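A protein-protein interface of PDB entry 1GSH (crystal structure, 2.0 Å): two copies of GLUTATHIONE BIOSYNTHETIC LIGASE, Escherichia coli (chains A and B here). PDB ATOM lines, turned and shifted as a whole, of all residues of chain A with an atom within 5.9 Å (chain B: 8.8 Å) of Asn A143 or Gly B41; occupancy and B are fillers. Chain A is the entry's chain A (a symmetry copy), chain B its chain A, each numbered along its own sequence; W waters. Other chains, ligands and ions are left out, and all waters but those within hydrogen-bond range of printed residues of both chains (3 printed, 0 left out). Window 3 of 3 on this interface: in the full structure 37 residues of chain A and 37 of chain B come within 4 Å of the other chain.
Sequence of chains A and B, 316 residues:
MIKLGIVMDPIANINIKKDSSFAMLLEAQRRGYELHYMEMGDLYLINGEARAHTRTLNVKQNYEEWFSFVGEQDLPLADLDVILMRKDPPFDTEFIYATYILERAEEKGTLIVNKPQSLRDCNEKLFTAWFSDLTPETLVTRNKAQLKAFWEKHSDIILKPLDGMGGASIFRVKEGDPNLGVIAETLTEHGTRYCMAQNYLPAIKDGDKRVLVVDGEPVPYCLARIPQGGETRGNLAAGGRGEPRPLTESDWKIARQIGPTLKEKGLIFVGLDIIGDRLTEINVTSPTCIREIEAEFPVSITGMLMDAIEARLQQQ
N of Asn A143 sits at hydrogen-bond distance from OG1 of Thr A141 (3.1 Å). The backbone carbonyl oxygen (O) of Arg B51 lies within hydrogen-bond range of the backbone NH (N) of Tyr B44 (2.9 Å). The side-chain amide nitrogen of Asn A143 lies within hydrogen-bond range of the side-chain amide oxygen of Gln A146, 3.0 Å away. OG1 of Thr A141 is in hydrogen-bond range of OE1 of Gln A146 (2.8 Å). OH of Tyr B44 lies within hydrogen-bond range of OD2 of Asp B74, 2.9 Å away.
Of the 19 printed residues of chain B, 5 touch a printed residue of chain A. Of the 11 printed residues of chain A, 4 touch a printed residue of chain B. Printed residues of chain A that touch a printed residue of chain B: Arg A142, Asn A143, Gln A146 and Tyr A194. Hydrophobic or aromatic side chains of chain A that line the printed part of chain B: Tyr A194. Among the printed residues, 8 pairs touch across the chains. Among the printed residues, Asp or Glu carboxylates within 4 Å of a Lys or Arg side-chain nitrogen of the other chain: Arg A142 with Glu B94 (3.0 Å).
No position is printed for both chains. Of the 8 pairs that touch across the chains among the printed residues, none has its exchanged pair printed and touching as well.
Of chain B, only Gly B41 comes within 4 Å of Asn A143. Gly B41 touches two residues of chain A. Of the printed residues of chain A, Met B40 touches Arg A142 (3.4 Å) and Tyr A194 (2.7 Å). Printed residues of chain B within 4 Å of Arg A142: Met B40, Gly B41 and Glu B94. Thr A188 touches none of the printed residues of chain B. Arg B55 touches none of the printed residues of chain A.
O of Gly B41 sits at hydrogen-bond distance from ND2 of Asn A143, at 3.0 Å. The backbone NH of Tyr A194 is in hydrogen-bond range of the side-chain carboxylate of Glu B94, at 2.9 Å. NH2 of Arg A142 is in salt-bridge range of OE1 of Glu B94, 3.0 Å away. The backbone carbonyl oxygen of Met B40 sits at hydrogen-bond distance from the side-chain hydroxyl of Tyr A194.
Water W1 bridges the side-chain carboxylate (OE2) of Glu B94 (2.7 Å) and the backbone carbonyl oxygen (O) of Tyr A194 (2.7 Å). Water W2 lies within hydrogen-bond range of the backbone carbonyl oxygen of Gly B41 (2.8 Å), the backbone carbonyl oxygen of Leu B43 (2.8 Å), the backbone NH of Arg A142 (2.9 Å) and the side-chain hydroxyl of Thr A141 (3.1 Å). Water W3 lies within hydrogen-bond range of ND2 of Asn A143, OE1 of Gln A146 and O of Asp B42.
Among the printed residues, merely in contact across the chains: Gln A146 with Tyr B44 (3.4 Å), Arg A142 with Met B40 (3.4 Å), Tyr A194 with Leu B43 (3.5 Å) and Arg A142 with Gly B41 (3.7 Å).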
ATOM      1  N   THR A 141       7.701   8.161   0.469  1.00  0.00           N
ATOM      2  CA  THR A 141       7.606   8.416  -0.960  1.00  0.00           C
ATOM      3  C   THR A 141       7.135   7.199  -1.739  1.00  0.00           C
ATOM      4  O   THR A 141       7.152   6.090  -1.227  1.00  0.00           O
ATOM      5  CB  THR A 141       9.015   8.895  -1.435  1.00  0.00           C
ATOM      6  OG1 THR A 141       8.918   9.284  -2.794  1.00  0.00           O
ATOM      7  CG2 THR A 141      10.076   7.816  -1.285  1.00  0.00           C
ATOM      8  N   ARG A 142       6.736   7.396  -3.004  1.00  0.00           N
ATOM      9  CA  ARG A 142       6.388   6.300  -3.902  1.00  0.00           C
ATOM     10  C   ARG A 142       7.556   6.117  -4.873  1.00  0.00           C
ATOM     11  O   ARG A 142       7.562   5.203  -5.682  1.00  0.00           O
ATOM     12  CB  ARG A 142       5.150   6.627  -4.728  1.00  0.00           C
ATOM     13  CG  ARG A 142       3.842   6.765  -3.955  1.00  0.00           C
ATOM     14  CD  ARG A 142       2.669   6.938  -4.895  1.00  0.00           C
ATOM     15  NE  ARG A 142       1.440   6.824  -4.121  1.00  0.00           N
ATOM     16  CZ  ARG A 142       0.202   6.950  -4.626  1.00  0.00           C
ATOM     17  NH1 ARG A 142      -0.074   7.201  -5.906  1.00  0.00           N
ATOM     18  NH2 ARG A 142      -0.818   6.840  -3.792  1.00  0.00           N
ATOM     19  N   ASN A 143       8.559   7.003  -4.851  1.00  0.00           N
ATOM     20  CA  ASN A 143       9.591   7.025  -5.876  1.00  0.00           C
ATOM     21  C   ASN A 143      10.882   6.339  -5.515  1.00  0.00           C
ATOM     22  O   ASN A 143      11.573   6.715  -4.584  1.00  0.00           O
ATOM     23  CB  ASN A 143       9.919   8.456  -6.252  1.00  0.00           C
ATOM     24  CG  ASN A 143       8.706   9.195  -6.809  1.00  0.00           C
ATOM     25  OD1 ASN A 143       7.963   8.708  -7.677  1.00  0.00           O
ATOM     26  ND2 ASN A 143       8.463  10.406  -6.310  1.00  0.00           N
ATOM     27  N   LYS A 144      11.191   5.350  -6.331  1.00  0.00           N
ATOM     28  CA  LYS A 144      12.376   4.535  -6.222  1.00  0.00           C
ATOM     29  C   LYS A 144      13.642   5.363  -6.277  1.00  0.00           C
ATOM     30  O   LYS A 144      14.593   5.110  -5.559  1.00  0.00           O
ATOM     31  CB  LYS A 144      12.310   3.578  -7.359  1.00  0.00           C
ATOM     32  CG  LYS A 144      13.295   2.458  -7.440  1.00  0.00           C
ATOM     33  CD  LYS A 144      12.813   1.813  -8.734  1.00  0.00           C
ATOM     34  CE  LYS A 144      13.398   0.447  -8.940  1.00  0.00           C
ATOM     35  NZ  LYS A 144      14.846   0.483  -8.823  1.00  0.00           N
ATOM     36  N   ALA A 145      13.624   6.403  -7.103  1.00  0.00           N
ATOM     37  CA  ALA A 145      14.773   7.275  -7.259  1.00  0.00           C
ATOM     38  C   ALA A 145      15.062   8.044  -5.991  1.00  0.00           C
ATOM     39  O   ALA A 145      16.233   8.256  -5.675  1.00  0.00           O
ATOM     40  CB  ALA A 145      14.509   8.241  -8.386  1.00  0.00           C
ATOM     41  N   GLN A 146      14.034   8.450  -5.233  1.00  0.00           N
ATOM     42  CA  GLN A 146      14.247   9.123  -3.954  1.00  0.00           C
ATOM     43  C   GLN A 146      14.721   8.130  -2.891  1.00  0.00           C
ATOM     44  O   GLN A 146      15.521   8.504  -2.033  1.00  0.00           O
ATOM     45  CB  GLN A 146      12.967   9.779  -3.446  1.00  0.00           C
ATOM     46  CG  GLN A 146      12.509  10.845  -4.414  1.00  0.00           C
ATOM     47  CD  GLN A 146      11.373  11.695  -3.892  1.00  0.00           C
ATOM     48  OE1 GLN A 146      10.191  11.445  -4.092  1.00  0.00           O
ATOM     49  NE2 GLN A 146      11.705  12.746  -3.185  1.00  0.00           N
ATOM     50  N   LEU A 147      14.261   6.866  -2.931  1.00  0.00           N
ATOM     51  CA  LEU A 147      14.694   5.861  -1.982  1.00  0.00           C
ATOM     52  C   LEU A 147      16.143   5.455  -2.204  1.00  0.00           C
ATOM     53  O   LEU A 147      16.869   5.124  -1.272  1.00  0.00           O
ATOM     54  CB  LEU A 147      13.819   4.645  -2.103  1.00  0.00           C
ATOM     55  CG  LEU A 147      12.399   4.764  -1.622  1.00  0.00           C
ATOM     56  CD1 LEU A 147      11.712   3.482  -1.996  1.00  0.00           C
ATOM     57  CD2 LEU A 147      12.351   5.054  -0.128  1.00  0.00           C
ATOM     58  N   LYS A 148      16.558   5.497  -3.459  1.00  0.00           N
ATOM     59  CA  LYS A 148      17.916   5.177  -3.877  1.00  0.00           C
ATOM     60  C   LYS A 148      18.814   6.269  -3.339  1.00  0.00           C
ATOM     61  O   LYS A 148      19.841   5.974  -2.734  1.00  0.00           O
ATOM     62  CB  LYS A 148      17.964   5.145  -5.392  1.00  0.00           C
ATOM     63  CG  LYS A 148      18.786   4.052  -6.003  1.00  0.00           C
ATOM     64  CD  LYS A 148      20.254   4.255  -5.711  1.00  0.00           C
ATOM     65  CE  LYS A 148      21.034   4.524  -7.004  1.00  0.00           C
ATOM     66  NZ  LYS A 148      22.436   4.736  -6.676  1.00  0.00           N
ATOM     67  N   THR A 188       6.333  -0.228  -2.793  1.00  0.00           N
ATOM     68  CA  THR A 188       5.600   0.852  -3.463  1.00  0.00           C
ATOM     69  C   THR A 188       4.639   0.316  -4.530  1.00  0.00           C
ATOM     70  O   THR A 188       3.949   1.074  -5.199  1.00  0.00           O
ATOM     71  CB  THR A 188       6.586   1.853  -4.141  1.00  0.00           C
ATOM     72  OG1 THR A 188       7.217   1.151  -5.208  1.00  0.00           O
ATOM     73  CG2 THR A 188       7.637   2.410  -3.205  1.00  0.00           C
ATOM     74  N   GLY A 191       5.507   1.774  -7.655  1.00  0.00           N
ATOM     75  CA  GLY A 191       5.316   3.201  -7.590  1.00  0.00           C
ATOM     76  C   GLY A 191       3.906   3.676  -7.383  1.00  0.00           C
ATOM     77  O   GLY A 191       3.649   4.860  -7.560  1.00  0.00           O
ATOM     78  N   TYR A 194       2.703   4.622  -1.267  1.00  0.00           N
ATOM     79  CA  TYR A 194       3.726   5.299  -0.494  1.00  0.00           C
ATOM     80  C   TYR A 194       4.391   4.304   0.422  1.00  0.00           C
ATOM     81  O   TYR A 194       3.689   3.415   0.873  1.00  0.00           O
ATOM     82  CB  TYR A 194       3.183   6.407   0.434  1.00  0.00           C
ATOM     83  CG  TYR A 194       2.600   7.610  -0.297  1.00  0.00           C
ATOM     84  CD1 TYR A 194       3.414   8.525  -0.954  1.00  0.00           C
ATOM     85  CD2 TYR A 194       1.206   7.757  -0.334  1.00  0.00           C
ATOM     86  CE1 TYR A 194       2.839   9.577  -1.671  1.00  0.00           C
ATOM     87  CE2 TYR A 194       0.620   8.799  -1.049  1.00  0.00           C
ATOM     88  CZ  TYR A 194       1.451   9.704  -1.703  1.00  0.00           C
ATOM     89  OH  TYR A 194       0.858  10.735  -2.391  1.00  0.00           O
ATOM     90  N   VAL B   7      -3.500  18.813  -7.328  1.00  0.00           N
ATOM     91  CA  VAL B   7      -3.133  17.404  -7.293  1.00  0.00           C
ATOM     92  C   VAL B   7      -4.257  16.692  -8.001  1.00  0.00           C
ATOM     93  O   VAL B   7      -5.418  16.802  -7.604  1.00  0.00           O
ATOM     94  CB  VAL B   7      -3.003  16.889  -5.862  1.00  0.00           C
ATOM     95  CG1 VAL B   7      -2.564  15.440  -5.834  1.00  0.00           C
ATOM     96  CG2 VAL B   7      -1.972  17.738  -5.163  1.00  0.00           C
ATOM     97  N   MET B   8      -3.964  15.960  -9.063  1.00  0.00           N
ATOM     98  CA  MET B   8      -5.049  15.342  -9.777  1.00  0.00           C
ATOM     99  C   MET B   8      -4.612  14.097 -10.502  1.00  0.00           C
ATOM    100  O   MET B   8      -3.422  13.799 -10.580  1.00  0.00           O
ATOM    101  CB  MET B   8      -5.641  16.366 -10.769  1.00  0.00           C
ATOM    102  CG  MET B   8      -4.687  16.835 -11.864  1.00  0.00           C
ATOM    103  SD  MET B   8      -5.409  18.115 -12.924  1.00  0.00           S
ATOM    104  CE  MET B   8      -6.430  17.237 -14.079  1.00  0.00           C
ATOM    105  N   MET B  38       0.625  18.617 -10.160  1.00  0.00           N
ATOM    106  CA  MET B  38       1.198  17.432  -9.588  1.00  0.00           C
ATOM    107  C   MET B  38       0.201  16.287  -9.466  1.00  0.00           C
ATOM    108  O   MET B  38      -1.008  16.447  -9.518  1.00  0.00           O
ATOM    109  CB  MET B  38       1.855  17.797  -8.236  1.00  0.00           C
ATOM    110  CG  MET B  38       1.005  18.350  -7.118  1.00  0.00           C
ATOM    111  SD  MET B  38       1.957  19.433  -6.025  1.00  0.00           S
ATOM    112  CE  MET B  38       0.804  20.776  -6.041  1.00  0.00           C
ATOM    113  N   GLU B  39       0.741  15.077  -9.485  1.00  0.00           N
ATOM    114  CA  GLU B  39       0.000  13.851  -9.260  1.00  0.00           C
ATOM    115  C   GLU B  39       0.355  13.317  -7.860  1.00  0.00           C
ATOM    116  O   GLU B  39       1.286  13.818  -7.219  1.00  0.00           O
ATOM    117  CB  GLU B  39       0.390  12.886 -10.353  1.00  0.00           C
ATOM    118  CG  GLU B  39      -0.111  13.370 -11.698  1.00  0.00           C
ATOM    119  CD  GLU B  39       0.438  12.604 -12.893  1.00  0.00           C
ATOM    120  OE1 GLU B  39       0.952  11.506 -12.712  1.00  0.00           O
ATOM    121  OE2 GLU B  39       0.357  13.096 -14.019  1.00  0.00           O
ATOM    122  N   MET B  40      -0.342  12.278  -7.363  1.00  0.00           N
ATOM    123  CA  MET B  40      -0.126  11.706  -6.039  1.00  0.00           C
ATOM    124  C   MET B  40       1.309  11.284  -5.788  1.00  0.00           C
ATOM    125  O   MET B  40       1.889  11.525  -4.730  1.00  0.00           O
ATOM    126  CB  MET B  40      -0.995  10.464  -5.834  1.00  0.00           C
ATOM    127  CG  MET B  40      -2.477  10.688  -5.810  1.00  0.00           C
ATOM    128  SD  MET B  40      -2.992  11.408  -4.245  1.00  0.00           S
ATOM    129  CE  MET B  40      -3.048   9.858  -3.386  1.00  0.00           C
ATOM    130  N   GLY B  41       1.908  10.641  -6.787  1.00  0.00           N
ATOM    131  CA  GLY B  41       3.280  10.153  -6.717  1.00  0.00           C
ATOM    132  C   GLY B  41       4.327  11.242  -6.610  1.00  0.00           C
ATOM    133  O   GLY B  41       5.484  10.936  -6.353  1.00  0.00           O
ATOM    134  N   ASP B  42       3.951  12.518  -6.818  1.00  0.00           N
ATOM    135  CA  ASP B  42       4.885  13.629  -6.756  1.00  0.00           C
ATOM    136  C   ASP B  42       5.085  14.183  -5.361  1.00  0.00           C
ATOM    137  O   ASP B  42       6.036  14.927  -5.101  1.00  0.00           O
ATOM    138  CB  ASP B  42       4.414  14.772  -7.665  1.00  0.00           C
ATOM    139  CG  ASP B  42       4.578  14.510  -9.156  1.00  0.00           C
ATOM    140  OD1 ASP B  42       5.550  13.903  -9.599  1.00  0.00           O
ATOM    141  OD2 ASP B  42       3.717  14.941  -9.899  1.00  0.00           O
ATOM    142  N   LEU B  43       4.155  13.835  -4.475  1.00  0.00           N
ATOM    143  CA  LEU B  43       4.145  14.342  -3.123  1.00  0.00           C
ATOM    144  C   LEU B  43       5.015  13.461  -2.234  1.00  0.00           C
ATOM    145  O   LEU B  43       5.029  12.236  -2.375  1.00  0.00           O
ATOM    146  CB  LEU B  43       2.694  14.356  -2.577  1.00  0.00           C
ATOM    147  CG  LEU B  43       1.495  14.987  -3.332  1.00  0.00           C
ATOM    148  CD1 LEU B  43       0.195  14.533  -2.659  1.00  0.00           C
ATOM    149  CD2 LEU B  43       1.604  16.499  -3.337  1.00  0.00           C
ATOM    150  N   TYR B  44       5.780  14.034  -1.317  1.00  0.00           N
ATOM    151  CA  TYR B  44       6.514  13.196  -0.410  1.00  0.00           C
ATOM    152  C   TYR B  44       6.734  13.977   0.845  1.00  0.00           C
ATOM    153  O   TYR B  44       6.405  15.155   0.929  1.00  0.00           O
ATOM    154  CB  TYR B  44       7.833  12.758  -1.074  1.00  0.00           C
ATOM    155  CG  TYR B  44       8.830  13.853  -1.403  1.00  0.00           C
ATOM    156  CD1 TYR B  44       8.734  14.624  -2.569  1.00  0.00           C
ATOM    157  CD2 TYR B  44       9.873  14.027  -0.508  1.00  0.00           C
ATOM    158  CE1 TYR B  44       9.700  15.585  -2.839  1.00  0.00           C
ATOM    159  CE2 TYR B  44      10.840  14.977  -0.767  1.00  0.00           C
ATOM    160  CZ  TYR B  44      10.748  15.743  -1.923  1.00  0.00           C
ATOM    161  OH  TYR B  44      11.774  16.637  -2.157  1.00  0.00           O
ATOM    162  N   LEU B  45       7.355  13.318   1.801  1.00  0.00           N
ATOM    163  CA  LEU B  45       7.520  13.917   3.111  1.00  0.00           C
ATOM    164  C   LEU B  45       8.945  13.633   3.531  1.00  0.00           C
ATOM    165  O   LEU B  45       9.350  12.488   3.465  1.00  0.00           O
ATOM    166  CB  LEU B  45       6.498  13.252   4.029  1.00  0.00           C
ATOM    167  CG  LEU B  45       5.883  13.877   5.255  1.00  0.00           C
ATOM    168  CD1 LEU B  45       5.218  15.201   4.950  1.00  0.00           C
ATOM    169  CD2 LEU B  45       4.802  12.913   5.753  1.00  0.00           C
ATOM    170  N   ARG B  51       6.777  18.195   0.608  1.00  0.00           N
ATOM    171  CA  ARG B  51       7.405  18.658  -0.616  1.00  0.00           C
ATOM    172  C   ARG B  51       6.827  17.948  -1.798  1.00  0.00           C
ATOM    173  O   ARG B  51       6.192  16.897  -1.679  1.00  0.00           O
ATOM    174  CB  ARG B  51       8.867  18.363  -0.673  1.00  0.00           C
ATOM    175  CG  ARG B  51       9.722  19.014   0.356  1.00  0.00           C
ATOM    176  CD  ARG B  51      11.072  18.996  -0.317  1.00  0.00           C
ATOM    177  NE  ARG B  51      11.859  19.980   0.355  1.00  0.00           N
ATOM    178  CZ  ARG B  51      12.436  20.983  -0.280  1.00  0.00           C
ATOM    179  NH1 ARG B  51      12.368  21.138  -1.591  1.00  0.00           N
ATOM    180  NH2 ARG B  51      12.986  21.929   0.481  1.00  0.00           N
ATOM    181  N   ALA B  52       7.057  18.552  -2.955  1.00  0.00           N
ATOM    182  CA  ALA B  52       6.654  17.933  -4.175  1.00  0.00           C
ATOM    183  C   ALA B  52       7.516  18.320  -5.334  1.00  0.00           C
ATOM    184  O   ALA B  52       8.167  19.354  -5.382  1.00  0.00           O
ATOM    185  CB  ALA B  52       5.270  18.312  -4.591  1.00  0.00           C
ATOM    186  N   HIS B  53       7.484  17.429  -6.293  1.00  0.00           N
ATOM    187  CA  HIS B  53       8.028  17.720  -7.609  1.00  0.00           C
ATOM    188  C   HIS B  53       6.884  18.381  -8.391  1.00  0.00           C
ATOM    189  O   HIS B  53       5.881  17.708  -8.617  1.00  0.00           O
ATOM    190  CB  HIS B  53       8.437  16.412  -8.265  1.00  0.00           C
ATOM    191  CG  HIS B  53       8.657  16.543  -9.757  1.00  0.00           C
ATOM    192  ND1 HIS B  53       7.970  15.956 -10.741  1.00  0.00           N
ATOM    193  CD2 HIS B  53       9.614  17.357 -10.311  1.00  0.00           C
ATOM    194  CE1 HIS B  53       8.470  16.387 -11.865  1.00  0.00           C
ATOM    195  NE2 HIS B  53       9.447  17.217 -11.584  1.00  0.00           N
ATOM    196  N   ARG B  55       5.394  20.734 -11.848  1.00  0.00           N
ATOM    197  CA  ARG B  55       5.661  21.113 -13.219  1.00  0.00           C
ATOM    198  C   ARG B  55       4.863  22.403 -13.387  1.00  0.00           C
ATOM    199  O   ARG B  55       3.685  22.437 -12.995  1.00  0.00           O
ATOM    200  CB  ARG B  55       5.139  20.083 -14.202  1.00  0.00           C
ATOM    201  CG  ARG B  55       6.174  19.053 -14.598  1.00  0.00           C
ATOM    202  CD  ARG B  55       5.858  17.728 -13.956  1.00  0.00           C
ATOM    203  NE  ARG B  55       5.223  16.777 -14.855  1.00  0.00           N
ATOM    204  CZ  ARG B  55       4.524  15.700 -14.427  1.00  0.00           C
ATOM    205  NH1 ARG B  55       4.350  15.395 -13.142  1.00  0.00           N
ATOM    206  NH2 ARG B  55       3.970  14.873 -15.313  1.00  0.00           N
ATOM    207  N   ASP B  74      11.419  21.081  -7.735  1.00  0.00           N
ATOM    208  CA  ASP B  74      11.166  20.411  -6.476  1.00  0.00           C
ATOM    209  C   ASP B  74      11.011  21.540  -5.479  1.00  0.00           C
ATOM    210  O   ASP B  74      11.933  22.349  -5.355  1.00  0.00           O
ATOM    211  CB  ASP B  74      12.345  19.564  -6.050  1.00  0.00           C
ATOM    212  CG  ASP B  74      12.074  18.749  -4.792  1.00  0.00           C
ATOM    213  OD1 ASP B  74      12.233  19.250  -3.689  1.00  0.00           O
ATOM    214  OD2 ASP B  74      11.695  17.598  -4.914  1.00  0.00           O
ATOM    215  N   LYS B  87      -8.085  14.828  -6.570  1.00  0.00           N
ATOM    216  CA  LYS B  87      -7.952  13.396  -6.805  1.00  0.00           C
ATOM    217  C   LYS B  87      -9.320  12.696  -6.792  1.00  0.00           C
ATOM    218  O   LYS B  87     -10.191  12.931  -5.943  1.00  0.00           O
ATOM    219  CB  LYS B  87      -7.013  12.847  -5.715  1.00  0.00           C
ATOM    220  CG  LYS B  87      -6.773  11.369  -5.804  1.00  0.00           C
ATOM    221  CD  LYS B  87      -6.037  11.022  -7.079  1.00  0.00           C
ATOM    222  CE  LYS B  87      -5.941   9.509  -7.212  1.00  0.00           C
ATOM    223  NZ  LYS B  87      -7.208   8.909  -7.623  1.00  0.00           N
ATOM    224  N   GLU B  94      -4.311   5.330   0.658  1.00  0.00           N
ATOM    225  CA  GLU B  94      -3.380   6.220  -0.036  1.00  0.00           C
ATOM    226  C   GLU B  94      -3.909   7.646  -0.063  1.00  0.00           C
ATOM    227  O   GLU B  94      -3.159   8.602   0.151  1.00  0.00           O
ATOM    228  CB  GLU B  94      -3.156   5.781  -1.470  1.00  0.00           C
ATOM    229  CG  GLU B  94      -2.421   4.462  -1.647  1.00  0.00           C
ATOM    230  CD  GLU B  94      -1.037   4.444  -0.978  1.00  0.00           C
ATOM    231  OE1 GLU B  94      -0.163   5.254  -1.299  1.00  0.00           O
ATOM    232  OE2 GLU B  94      -0.833   3.608  -0.111  1.00  0.00           O
ATOM    233  N   ALA B  98      -2.037  10.905   1.672  1.00  0.00           N
ATOM    234  CA  ALA B  98      -1.775  12.160   0.963  1.00  0.00           C
ATOM    235  C   ALA B  98      -2.335  13.356   1.703  1.00  0.00           C
ATOM    236  O   ALA B  98      -1.818  14.469   1.671  1.00  0.00           O
ATOM    237  CB  ALA B  98      -2.402  12.142  -0.405  1.00  0.00           C
ATOM    238  N   ILE B 101       0.124  14.592   4.199  1.00  0.00           N
ATOM    239  CA  ILE B 101       1.164  15.343   3.507  1.00  0.00           C
ATOM    240  C   ILE B 101       0.646  16.752   3.226  1.00  0.00           C
ATOM    241  O   ILE B 101       1.300  17.747   3.545  1.00  0.00           O
ATOM    242  CB  ILE B 101       1.534  14.573   2.210  1.00  0.00           C
ATOM    243  CG1 ILE B 101       2.202  13.246   2.560  1.00  0.00           C
ATOM    244  CG2 ILE B 101       2.453  15.422   1.354  1.00  0.00           C
ATOM    245  CD1 ILE B 101       2.491  12.364   1.330  1.00  0.00           C
HETATM  246  O   HOH W   1       1.127   2.572   1.366  1.00  0.00           O
HETATM  247  O   HOH W   2       6.038  10.047  -3.785  1.00  0.00           O
HETATM  248  O   HOH W   3       8.830  13.369  -6.068  1.00  0.00           O
